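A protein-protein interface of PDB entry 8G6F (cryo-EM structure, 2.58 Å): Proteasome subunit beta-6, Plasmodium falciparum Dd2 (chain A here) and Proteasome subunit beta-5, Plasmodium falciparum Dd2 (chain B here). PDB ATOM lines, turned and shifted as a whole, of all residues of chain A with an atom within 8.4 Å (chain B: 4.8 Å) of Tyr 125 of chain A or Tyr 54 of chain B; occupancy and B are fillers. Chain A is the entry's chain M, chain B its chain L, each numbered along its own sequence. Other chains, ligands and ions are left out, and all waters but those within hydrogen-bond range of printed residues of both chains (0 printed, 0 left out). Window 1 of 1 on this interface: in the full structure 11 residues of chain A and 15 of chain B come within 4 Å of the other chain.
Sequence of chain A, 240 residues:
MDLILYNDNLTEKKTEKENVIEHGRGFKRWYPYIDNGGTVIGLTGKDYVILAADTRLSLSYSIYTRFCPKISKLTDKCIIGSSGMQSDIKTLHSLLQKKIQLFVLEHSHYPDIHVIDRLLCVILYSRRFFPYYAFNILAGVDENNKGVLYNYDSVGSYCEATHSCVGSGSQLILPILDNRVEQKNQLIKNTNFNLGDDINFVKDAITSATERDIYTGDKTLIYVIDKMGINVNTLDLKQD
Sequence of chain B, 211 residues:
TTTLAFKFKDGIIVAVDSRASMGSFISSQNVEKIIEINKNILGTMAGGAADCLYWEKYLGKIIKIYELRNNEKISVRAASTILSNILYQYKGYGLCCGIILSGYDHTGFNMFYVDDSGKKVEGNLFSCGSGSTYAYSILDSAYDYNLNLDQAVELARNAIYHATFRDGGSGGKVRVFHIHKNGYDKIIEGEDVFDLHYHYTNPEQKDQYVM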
ATOM      1  N   LEU A  92      25.399  14.759  -7.610  1.00  0.00           N
ATOM      2  CA  LEU A  92      24.121  15.236  -8.120  1.00  0.00           C
ATOM      3  C   LEU A  92      24.011  15.031  -9.624  1.00  0.00           C
ATOM      4  O   LEU A  92      22.956  14.629 -10.124  1.00  0.00           O
ATOM      5  CB  LEU A  92      23.942  16.708  -7.760  1.00  0.00           C
ATOM      6  CG  LEU A  92      22.614  17.354  -8.147  1.00  0.00           C
ATOM      7  CD1 LEU A  92      21.507  16.905  -7.218  1.00  0.00           C
ATOM      8  CD2 LEU A  92      22.753  18.857  -8.128  1.00  0.00           C
ATOM      9  N   ARG A 118      11.865  19.754 -13.426  1.00  0.00           N
ATOM     10  CA  ARG A 118      11.033  19.288 -12.319  1.00  0.00           C
ATOM     11  C   ARG A 118      11.708  18.139 -11.577  1.00  0.00           C
ATOM     12  O   ARG A 118      11.670  18.072 -10.340  1.00  0.00           O
ATOM     13  CB  ARG A 118       9.657  18.874 -12.835  1.00  0.00           C
ATOM     14  CG  ARG A 118       8.696  18.397 -11.756  1.00  0.00           C
ATOM     15  CD  ARG A 118       8.302  19.500 -10.790  1.00  0.00           C
ATOM     16  NE  ARG A 118       7.490  20.528 -11.432  1.00  0.00           N
ATOM     17  CZ  ARG A 118       6.189  20.706 -11.240  1.00  0.00           C
ATOM     18  NH1 ARG A 118       5.488  19.919 -10.438  1.00  0.00           N
ATOM     19  NH2 ARG A 118       5.572  21.702 -11.867  1.00  0.00           N
ATOM     20  N   LEU A 119      12.336  17.227 -12.319  1.00  0.00           N
ATOM     21  CA  LEU A 119      13.037  16.111 -11.697  1.00  0.00           C
ATOM     22  C   LEU A 119      14.147  16.607 -10.781  1.00  0.00           C
ATOM     23  O   LEU A 119      14.289  16.142  -9.643  1.00  0.00           O
ATOM     24  CB  LEU A 119      13.603  15.202 -12.788  1.00  0.00           C
ATOM     25  CG  LEU A 119      14.034  13.782 -12.433  1.00  0.00           C
ATOM     26  CD1 LEU A 119      13.018  13.086 -11.545  1.00  0.00           C
ATOM     27  CD2 LEU A 119      14.253  12.998 -13.711  1.00  0.00           C
ATOM     28  N   LEU A 120      14.942  17.560 -11.266  1.00  0.00           N
ATOM     29  CA  LEU A 120      16.021  18.115 -10.461  1.00  0.00           C
ATOM     30  C   LEU A 120      15.476  18.848  -9.244  1.00  0.00           C
ATOM     31  O   LEU A 120      16.083  18.814  -8.172  1.00  0.00           O
ATOM     32  CB  LEU A 120      16.876  19.048 -11.317  1.00  0.00           C
ATOM     33  CG  LEU A 120      18.110  19.673 -10.670  1.00  0.00           C
ATOM     34  CD1 LEU A 120      18.995  18.620 -10.036  1.00  0.00           C
ATOM     35  CD2 LEU A 120      18.883  20.464 -11.696  1.00  0.00           C
ATOM     36  N   CYS A 121      14.337  19.525  -9.392  1.00  0.00           N
ATOM     37  CA  CYS A 121      13.729  20.196  -8.247  1.00  0.00           C
ATOM     38  C   CYS A 121      13.356  19.199  -7.163  1.00  0.00           C
ATOM     39  O   CYS A 121      13.584  19.444  -5.971  1.00  0.00           O
ATOM     40  CB  CYS A 121      12.490  20.971  -8.685  1.00  0.00           C
ATOM     41  SG  CYS A 121      12.817  22.612  -9.301  1.00  0.00           S
ATOM     42  N   VAL A 122      12.759  18.076  -7.555  1.00  0.00           N
ATOM     43  CA  VAL A 122      12.416  17.048  -6.576  1.00  0.00           C
ATOM     44  C   VAL A 122      13.680  16.513  -5.915  1.00  0.00           C
ATOM     45  O   VAL A 122      13.757  16.387  -4.686  1.00  0.00           O
ATOM     46  CB  VAL A 122      11.605  15.924  -7.247  1.00  0.00           C
ATOM     47  CG1 VAL A 122      11.591  14.678  -6.380  1.00  0.00           C
ATOM     48  CG2 VAL A 122      10.193  16.395  -7.533  1.00  0.00           C
ATOM     49  N   ILE A 123      14.697  16.207  -6.724  1.00  0.00           N
ATOM     50  CA  ILE A 123      15.950  15.688  -6.181  1.00  0.00           C
ATOM     51  C   ILE A 123      16.540  16.663  -5.173  1.00  0.00           C
ATOM     52  O   ILE A 123      17.064  16.260  -4.129  1.00  0.00           O
ATOM     53  CB  ILE A 123      16.947  15.397  -7.318  1.00  0.00           C
ATOM     54  CG1 ILE A 123      16.548  14.130  -8.069  1.00  0.00           C
ATOM     55  CG2 ILE A 123      18.357  15.273  -6.770  1.00  0.00           C
ATOM     56  CD1 ILE A 123      17.296  13.932  -9.365  1.00  0.00           C
ATOM     57  N   LEU A 124      16.485  17.958  -5.476  1.00  0.00           N
ATOM     58  CA  LEU A 124      17.132  18.946  -4.626  1.00  0.00           C
ATOM     59  C   LEU A 124      16.356  19.176  -3.340  1.00  0.00           C
ATOM     60  O   LEU A 124      16.958  19.319  -2.273  1.00  0.00           O
ATOM     61  CB  LEU A 124      17.301  20.259  -5.386  1.00  0.00           C
ATOM     62  CG  LEU A 124      18.403  20.279  -6.443  1.00  0.00           C
ATOM     63  CD1 LEU A 124      18.414  21.611  -7.155  1.00  0.00           C
ATOM     64  CD2 LEU A 124      19.751  20.000  -5.824  1.00  0.00           C
ATOM     65  N   TYR A 125      15.026  19.223  -3.412  1.00  0.00           N
ATOM     66  CA  TYR A 125      14.255  19.407  -2.192  1.00  0.00           C
ATOM     67  C   TYR A 125      14.225  18.151  -1.333  1.00  0.00           C
ATOM     68  O   TYR A 125      13.921  18.245  -0.141  1.00  0.00           O
ATOM     69  CB  TYR A 125      12.828  19.846  -2.508  1.00  0.00           C
ATOM     70  CG  TYR A 125      12.234  20.687  -1.407  1.00  0.00           C
ATOM     71  CD1 TYR A 125      12.404  22.059  -1.391  1.00  0.00           C
ATOM     72  CD2 TYR A 125      11.521  20.107  -0.373  1.00  0.00           C
ATOM     73  CE1 TYR A 125      11.875  22.829  -0.386  1.00  0.00           C
ATOM     74  CE2 TYR A 125      10.990  20.869   0.636  1.00  0.00           C
ATOM     75  CZ  TYR A 125      11.169  22.230   0.624  1.00  0.00           C
ATOM     76  OH  TYR A 125      10.640  22.999   1.629  1.00  0.00           O
ATOM     77  N   SER A 126      14.536  16.983  -1.896  1.00  0.00           N
ATOM     78  CA  SER A 126      14.609  15.786  -1.065  1.00  0.00           C
ATOM     79  C   SER A 126      15.620  15.952   0.062  1.00  0.00           C
ATOM     80  O   SER A 126      15.489  15.315   1.111  1.00  0.00           O
ATOM     81  CB  SER A 126      14.964  14.572  -1.921  1.00  0.00           C
ATOM     82  OG  SER A 126      16.354  14.511  -2.166  1.00  0.00           O
ATOM     83  N   ARG A 127      16.625  16.802  -0.131  1.00  0.00           N
ATOM     84  CA  ARG A 127      17.651  17.075   0.869  1.00  0.00           C
ATOM     85  C   ARG A 127      17.531  18.497   1.411  1.00  0.00           C
ATOM     86  O   ARG A 127      18.525  19.162   1.689  1.00  0.00           O
ATOM     87  CB  ARG A 127      19.037  16.838   0.281  1.00  0.00           C
ATOM     88  CG  ARG A 127      19.657  15.533   0.711  1.00  0.00           C
ATOM     89  CD  ARG A 127      20.686  15.072  -0.275  1.00  0.00           C
ATOM     90  NE  ARG A 127      21.862  15.931  -0.274  1.00  0.00           N
ATOM     91  CZ  ARG A 127      22.817  15.890   0.642  1.00  0.00           C
ATOM     92  NH1 ARG A 127      22.753  15.061   1.670  1.00  0.00           N
ATOM     93  NH2 ARG A 127      23.865  16.698   0.522  1.00  0.00           N
ATOM     94  N   ARG A 128      16.294  18.963   1.587  1.00  0.00           N
ATOM     95  CA  ARG A 128      16.060  20.357   1.942  1.00  0.00           C
ATOM     96  C   ARG A 128      16.745  20.738   3.248  1.00  0.00           C
ATOM     97  O   ARG A 128      17.091  21.907   3.446  1.00  0.00           O
ATOM     98  CB  ARG A 128      14.555  20.611   2.029  1.00  0.00           C
ATOM     99  CG  ARG A 128      14.155  21.891   2.730  1.00  0.00           C
ATOM    100  CD  ARG A 128      14.681  23.111   2.009  1.00  0.00           C
ATOM    101  NE  ARG A 128      14.306  24.343   2.690  1.00  0.00           N
ATOM    102  CZ  ARG A 128      14.828  24.754   3.836  1.00  0.00           C
ATOM    103  NH1 ARG A 128      15.762  24.058   4.459  1.00  0.00           N
ATOM    104  NH2 ARG A 128      14.400  25.892   4.371  1.00  0.00           N
ATOM    105  N   PHE A 129      16.943  19.783   4.150  1.00  0.00           N
ATOM    106  CA  PHE A 129      17.492  20.061   5.470  1.00  0.00           C
ATOM    107  C   PHE A 129      18.959  19.671   5.592  1.00  0.00           C
ATOM    108  O   PHE A 129      19.499  19.656   6.701  1.00  0.00           O
ATOM    109  CB  PHE A 129      16.641  19.357   6.523  1.00  0.00           C
ATOM    110  CG  PHE A 129      15.176  19.628   6.364  1.00  0.00           C
ATOM    111  CD1 PHE A 129      14.681  20.908   6.522  1.00  0.00           C
ATOM    112  CD2 PHE A 129      14.302  18.617   6.018  1.00  0.00           C
ATOM    113  CE1 PHE A 129      13.341  21.170   6.360  1.00  0.00           C
ATOM    114  CE2 PHE A 129      12.959  18.874   5.855  1.00  0.00           C
ATOM    115  CZ  PHE A 129      12.479  20.151   6.025  1.00  0.00           C
ATOM    116  N   PHE A 130      19.608  19.359   4.475  1.00  0.00           N
ATOM    117  CA  PHE A 130      21.046  19.159   4.362  1.00  0.00           C
ATOM    118  C   PHE A 130      21.393  19.342   2.891  1.00  0.00           C
ATOM    119  O   PHE A 130      21.853  18.402   2.235  1.00  0.00           O
ATOM    120  CB  PHE A 130      21.456  17.776   4.867  1.00  0.00           C
ATOM    121  CG  PHE A 130      22.932  17.625   5.090  1.00  0.00           C
ATOM    122  CD1 PHE A 130      23.598  18.429   5.993  1.00  0.00           C
ATOM    123  CD2 PHE A 130      23.654  16.673   4.396  1.00  0.00           C
ATOM    124  CE1 PHE A 130      24.953  18.285   6.196  1.00  0.00           C
ATOM    125  CE2 PHE A 130      25.009  16.527   4.596  1.00  0.00           C
ATOM    126  CZ  PHE A 130      25.658  17.332   5.495  1.00  0.00           C
ATOM    127  N   PRO A 131      21.190  20.538   2.344  1.00  0.00           N
ATOM    128  CA  PRO A 131      21.157  20.689   0.885  1.00  0.00           C
ATOM    129  C   PRO A 131      22.490  20.381   0.223  1.00  0.00           C
ATOM    130  O   PRO A 131      23.558  20.514   0.822  1.00  0.00           O
ATOM    131  CB  PRO A 131      20.773  22.160   0.687  1.00  0.00           C
ATOM    132  CG  PRO A 131      20.391  22.678   2.014  1.00  0.00           C
ATOM    133  CD  PRO A 131      21.010  21.817   3.041  1.00  0.00           C
ATOM    134  N   TYR A 132      22.408  19.958  -1.037  1.00  0.00           N
ATOM    135  CA  TYR A 132      23.588  19.916  -1.884  1.00  0.00           C
ATOM    136  C   TYR A 132      24.200  21.304  -1.961  1.00  0.00           C
ATOM    137  O   TYR A 132      23.505  22.285  -2.233  1.00  0.00           O
ATOM    138  CB  TYR A 132      23.227  19.445  -3.293  1.00  0.00           C
ATOM    139  CG  TYR A 132      22.785  18.009  -3.407  1.00  0.00           C
ATOM    140  CD1 TYR A 132      23.708  16.994  -3.589  1.00  0.00           C
ATOM    141  CD2 TYR A 132      21.443  17.674  -3.360  1.00  0.00           C
ATOM    142  CE1 TYR A 132      23.309  15.686  -3.703  1.00  0.00           C
ATOM    143  CE2 TYR A 132      21.034  16.369  -3.475  1.00  0.00           C
ATOM    144  CZ  TYR A 132      21.969  15.378  -3.645  1.00  0.00           C
ATOM    145  OH  TYR A 132      21.562  14.072  -3.760  1.00  0.00           O
ATOM    146  N   SER A 154      20.277  25.638  -5.318  1.00  0.00           N
ATOM    147  CA  SER A 154      20.576  24.482  -4.485  1.00  0.00           C
ATOM    148  C   SER A 154      19.355  23.894  -3.790  1.00  0.00           C
ATOM    149  O   SER A 154      19.475  22.858  -3.131  1.00  0.00           O
ATOM    150  CB  SER A 154      21.626  24.853  -3.436  1.00  0.00           C
ATOM    151  OG  SER A 154      21.040  25.495  -2.317  1.00  0.00           O
ATOM    152  N   VAL A 155      18.188  24.528  -3.894  1.00  0.00           N
ATOM    153  CA  VAL A 155      16.968  23.854  -3.458  1.00  0.00           C
ATOM    154  C   VAL A 155      15.815  24.057  -4.436  1.00  0.00           C
ATOM    155  O   VAL A 155      14.875  23.258  -4.466  1.00  0.00           O
ATOM    156  CB  VAL A 155      16.571  24.315  -2.045  1.00  0.00           C
ATOM    157  CG1 VAL A 155      15.237  23.719  -1.648  1.00  0.00           C
ATOM    158  CG2 VAL A 155      17.639  23.923  -1.047  1.00  0.00           C
ATOM    159  N   GLY A 156      15.877  25.105  -5.253  1.00  0.00           N
ATOM    160  CA  GLY A 156      14.724  25.493  -6.047  1.00  0.00           C
ATOM    161  C   GLY A 156      15.129  26.101  -7.369  1.00  0.00           C
ATOM    162  O   GLY A 156      16.276  26.509  -7.562  1.00  0.00           O
ATOM    163  N   SER A 157      14.155  26.191  -8.270  1.00  0.00           N
ATOM    164  CA  SER A 157      14.396  26.496  -9.672  1.00  0.00           C
ATOM    165  C   SER A 157      13.710  27.784 -10.094  1.00  0.00           C
ATOM    166  O   SER A 157      12.657  28.146  -9.564  1.00  0.00           O
ATOM    167  CB  SER A 157      13.893  25.377 -10.568  1.00  0.00           C
ATOM    168  OG  SER A 157      14.135  25.681 -11.926  1.00  0.00           O
ATOM    169  N   ALA B  50      12.102  28.722  -2.713  1.00  0.00           N
ATOM    170  CA  ALA B  50      12.073  27.283  -2.939  1.00  0.00           C
ATOM    171  C   ALA B  50      11.015  26.610  -2.078  1.00  0.00           C
ATOM    172  O   ALA B  50      10.264  25.755  -2.562  1.00  0.00           O
ATOM    173  CB  ALA B  50      13.449  26.684  -2.661  1.00  0.00           C
ATOM    174  N   ASP B  51      10.943  26.982  -0.799  1.00  0.00           N
ATOM    175  CA  ASP B  51       9.939  26.404   0.088  1.00  0.00           C
ATOM    176  C   ASP B  51       8.536  26.716  -0.406  1.00  0.00           C
ATOM    177  O   ASP B  51       7.676  25.830  -0.484  1.00  0.00           O
ATOM    178  CB  ASP B  51      10.129  26.937   1.506  1.00  0.00           C
ATOM    179  CG  ASP B  51      11.442  26.520   2.109  1.00  0.00           C
ATOM    180  OD1 ASP B  51      12.009  25.510   1.650  1.00  0.00           O
ATOM    181  OD2 ASP B  51      11.909  27.201   3.040  1.00  0.00           O
ATOM    182  N   CYS B  52       8.292  27.978  -0.757  1.00  0.00           N
ATOM    183  CA  CYS B  52       6.977  28.368  -1.241  1.00  0.00           C
ATOM    184  C   CYS B  52       6.603  27.579  -2.487  1.00  0.00           C
ATOM    185  O   CYS B  52       5.508  27.015  -2.570  1.00  0.00           O
ATOM    186  CB  CYS B  52       6.950  29.867  -1.528  1.00  0.00           C
ATOM    187  SG  CYS B  52       6.929  30.914  -0.061  1.00  0.00           S
ATOM    188  N   LEU B  53       7.506  27.514  -3.465  1.00  0.00           N
ATOM    189  CA  LEU B  53       7.185  26.834  -4.712  1.00  0.00           C
ATOM    190  C   LEU B  53       6.929  25.350  -4.484  1.00  0.00           C
ATOM    191  O   LEU B  53       5.948  24.793  -4.996  1.00  0.00           O
ATOM    192  CB  LEU B  53       8.315  27.038  -5.718  1.00  0.00           C
ATOM    193  CG  LEU B  53       8.463  28.467  -6.243  1.00  0.00           C
ATOM    194  CD1 LEU B  53       9.751  28.618  -7.026  1.00  0.00           C
ATOM    195  CD2 LEU B  53       7.275  28.857  -7.096  1.00  0.00           C
ATOM    196  N   TYR B  54       7.787  24.693  -3.701  1.00  0.00           N
ATOM    197  CA  TYR B  54       7.620  23.264  -3.487  1.00  0.00           C
ATOM    198  C   TYR B  54       6.305  22.967  -2.784  1.00  0.00           C
ATOM    199  O   TYR B  54       5.571  22.052  -3.173  1.00  0.00           O
ATOM    200  CB  TYR B  54       8.785  22.708  -2.678  1.00  0.00           C
ATOM    201  CG  TYR B  54       8.633  21.236  -2.398  1.00  0.00           C
ATOM    202  CD1 TYR B  54       9.065  20.291  -3.315  1.00  0.00           C
ATOM    203  CD2 TYR B  54       8.039  20.790  -1.231  1.00  0.00           C
ATOM    204  CE1 TYR B  54       8.920  18.950  -3.071  1.00  0.00           C
ATOM    205  CE2 TYR B  54       7.891  19.453  -0.980  1.00  0.00           C
ATOM    206  CZ  TYR B  54       8.332  18.535  -1.902  1.00  0.00           C
ATOM    207  OH  TYR B  54       8.185  17.193  -1.650  1.00  0.00           O
ATOM    208  N   TRP B  55       5.985  23.729  -1.739  1.00  0.00           N
ATOM    209  CA  TRP B  55       4.792  23.406  -0.977  1.00  0.00           C
ATOM    210  C   TRP B  55       3.522  23.816  -1.706  1.00  0.00           C
ATOM    211  O   TRP B  55       2.487  23.164  -1.541  1.00  0.00           O
ATOM    212  CB  TRP B  55       4.883  24.041   0.407  1.00  0.00           C
ATOM    213  CG  TRP B  55       5.923  23.355   1.232  1.00  0.00           C
ATOM    214  CD1 TRP B  55       7.064  23.899   1.733  1.00  0.00           C
ATOM    215  CD2 TRP B  55       5.930  21.978   1.625  1.00  0.00           C
ATOM    216  NE1 TRP B  55       7.779  22.953   2.420  1.00  0.00           N
ATOM    217  CE2 TRP B  55       7.104  21.764   2.370  1.00  0.00           C
ATOM    218  CE3 TRP B  55       5.056  20.906   1.424  1.00  0.00           C
ATOM    219  CZ2 TRP B  55       7.424  20.526   2.917  1.00  0.00           C
ATOM    220  CZ3 TRP B  55       5.376  19.679   1.966  1.00  0.00           C
ATOM    221  CH2 TRP B  55       6.551  19.499   2.703  1.00  0.00           C
ATOM    222  N   GLU B  56       3.579  24.838  -2.559  1.00  0.00           N
ATOM    223  CA  GLU B  56       2.429  25.122  -3.406  1.00  0.00           C
ATOM    224  C   GLU B  56       2.207  24.010  -4.419  1.00  0.00           C
ATOM    225  O   GLU B  56       1.060  23.651  -4.708  1.00  0.00           O
ATOM    226  CB  GLU B  56       2.603  26.458  -4.122  1.00  0.00           C
ATOM    227  CG  GLU B  56       2.621  27.689  -3.221  1.00  0.00           C
ATOM    228  CD  GLU B  56       1.866  27.504  -1.922  1.00  0.00           C
ATOM    229  OE1 GLU B  56       0.681  27.115  -1.967  1.00  0.00           O
ATOM    230  OE2 GLU B  56       2.464  27.739  -0.852  1.00  0.00           O
ATOM    231  N   LYS B  57       3.281  23.451  -4.980  1.00  0.00           N
ATOM    232  CA  LYS B  57       3.110  22.322  -5.888  1.00  0.00           C
ATOM    233  C   LYS B  57       2.534  21.114  -5.156  1.00  0.00           C
ATOM    234  O   LYS B  57       1.679  20.399  -5.693  1.00  0.00           O
ATOM    235  CB  LYS B  57       4.441  21.975  -6.545  1.00  0.00           C
ATOM    236  CG  LYS B  57       4.879  22.985  -7.584  1.00  0.00           C
ATOM    237  CD  LYS B  57       6.191  22.578  -8.232  1.00  0.00           C
ATOM    238  CE  LYS B  57       7.213  23.706  -8.249  1.00  0.00           C
ATOM    239  NZ  LYS B  57       8.361  23.421  -7.342  1.00  0.00           N
ATOM    240  N   TYR B  58       2.996  20.871  -3.932  1.00  0.00           N
ATOM    241  CA  TYR B  58       2.445  19.791  -3.118  1.00  0.00           C
ATOM    242  C   TYR B  58       0.950  19.986  -2.887  1.00  0.00           C
ATOM    243  O   TYR B  58       0.149  19.054  -3.049  1.00  0.00           O
ATOM    244  CB  TYR B  58       3.196  19.745  -1.791  1.00  0.00           C
ATOM    245  CG  TYR B  58       3.086  18.453  -1.030  1.00  0.00           C
ATOM    246  CD1 TYR B  58       3.804  17.333  -1.416  1.00  0.00           C
ATOM    247  CD2 TYR B  58       2.279  18.358   0.092  1.00  0.00           C
ATOM    248  CE1 TYR B  58       3.713  16.156  -0.714  1.00  0.00           C
ATOM    249  CE2 TYR B  58       2.183  17.189   0.799  1.00  0.00           C
ATOM    250  CZ  TYR B  58       2.900  16.088   0.396  1.00  0.00           C
ATOM    251  OH  TYR B  58       2.799  14.915   1.105  1.00  0.00           O
ATOM    252  N   LEU B  95      11.678  26.412   7.589  1.00  0.00           N
ATOM    253  CA  LEU B  95      10.880  26.809   6.440  1.00  0.00           C
ATOM    254  C   LEU B  95      10.532  28.288   6.528  1.00  0.00           C
ATOM    255  O   LEU B  95      10.275  28.819   7.611  1.00  0.00           O
ATOM    256  CB  LEU B  95       9.600  25.978   6.366  1.00  0.00           C
ATOM    257  CG  LEU B  95       9.751  24.484   6.080  1.00  0.00           C
ATOM    258  CD1 LEU B  95       8.387  23.858   5.885  1.00  0.00           C
ATOM    259  CD2 LEU B  95      10.627  24.240   4.866  1.00  0.00           C
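Printed residues of chain B within 4 Å of Tyr 125 of chain A: Ala 50 (3.99 Å), Asp 51 (2.9 Å), Tyr 54 (3.5 Å), Trp 55 (3.0 Å) and Leu 95 (3.5 Å).
Tyr 54 of chain B touches one residue of chain A.
Printed residues of chain A within 4 Å of Trp 55 of chain B: Tyr 125.
Printed residues of chain A within 4 Å of Leu 53 of chain B: Ser 157 (3.9 Å).
Printed residues of chain B within 4 Å of Val 155 of chain A: Ala 50.
Of the printed residues of chain A, Leu 95 of chain B touches Tyr 125.
Arg 127 of chain A touches none of the printed residues of chain B.
Tyr 132 of chain A touches none of the printed residues of chain B.
The nearest printed residue of chain B that does not touch Ser 157 of chain A is Ala 50 of chain B (5.7 Å).
The guanidinium group (NE) of Arg 128 of chain A is in salt-bridge range of the side-chain carboxylate (OD1) of Asp 51 of chain B.
The side-chain hydroxyl (OH) of Tyr 125 of chain A sits at hydrogen-bond distance from the indole nitrogen (NE1) of Trp 55 of chain B.
OD1 of Asp 51 of chain B lies within hydrogen-bond range of OH of Tyr 125 of chain A (2.9 Å).
Hydrophobic or aromatic side chains of chain A within 4 Å of the printed part of chain B: Tyr 125 and Val 155.
Of the 10 printed residues of chain B, 7 touch a printed residue of chain A.
Hydrophobic or aromatic side chains of chain B that line the printed part of chain A: Ala 50, Leu 53, Tyr 54, Trp 55 and Leu 95.
Along chain B the printed residues that touch a printed residue of chain A span positions 50 to 95.
Among the printed residues, Asp or Glu carboxylates within 4 Å of a Lys or Arg side-chain nitrogen of the other chain: Arg 128 of chain A with Asp 51 of chain B.
Arg 118 of chain A touches Lys 57 of chain B (NH1 to CD, 3.5 Å).
Tyr 125 of chain A touches Ala 50 of chain B (CE1 to O, 3.99 Å).
CD2 of Tyr 54 of chain B touches CE2 of Tyr 125 of chain A (3.5 Å).
Tyr 125 of chain A touches Leu 95 of chain B (OH to CD2, 3.5 Å).
CG1 of Val 155 of chain A touches CB of Ala 50 of chain B (3.6 Å).
Ala 50 of chain B touches Gly 156 of chain A (CB to CA, 3.8 Å).
Ser 157 of chain A touches Leu 53 of chain B.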
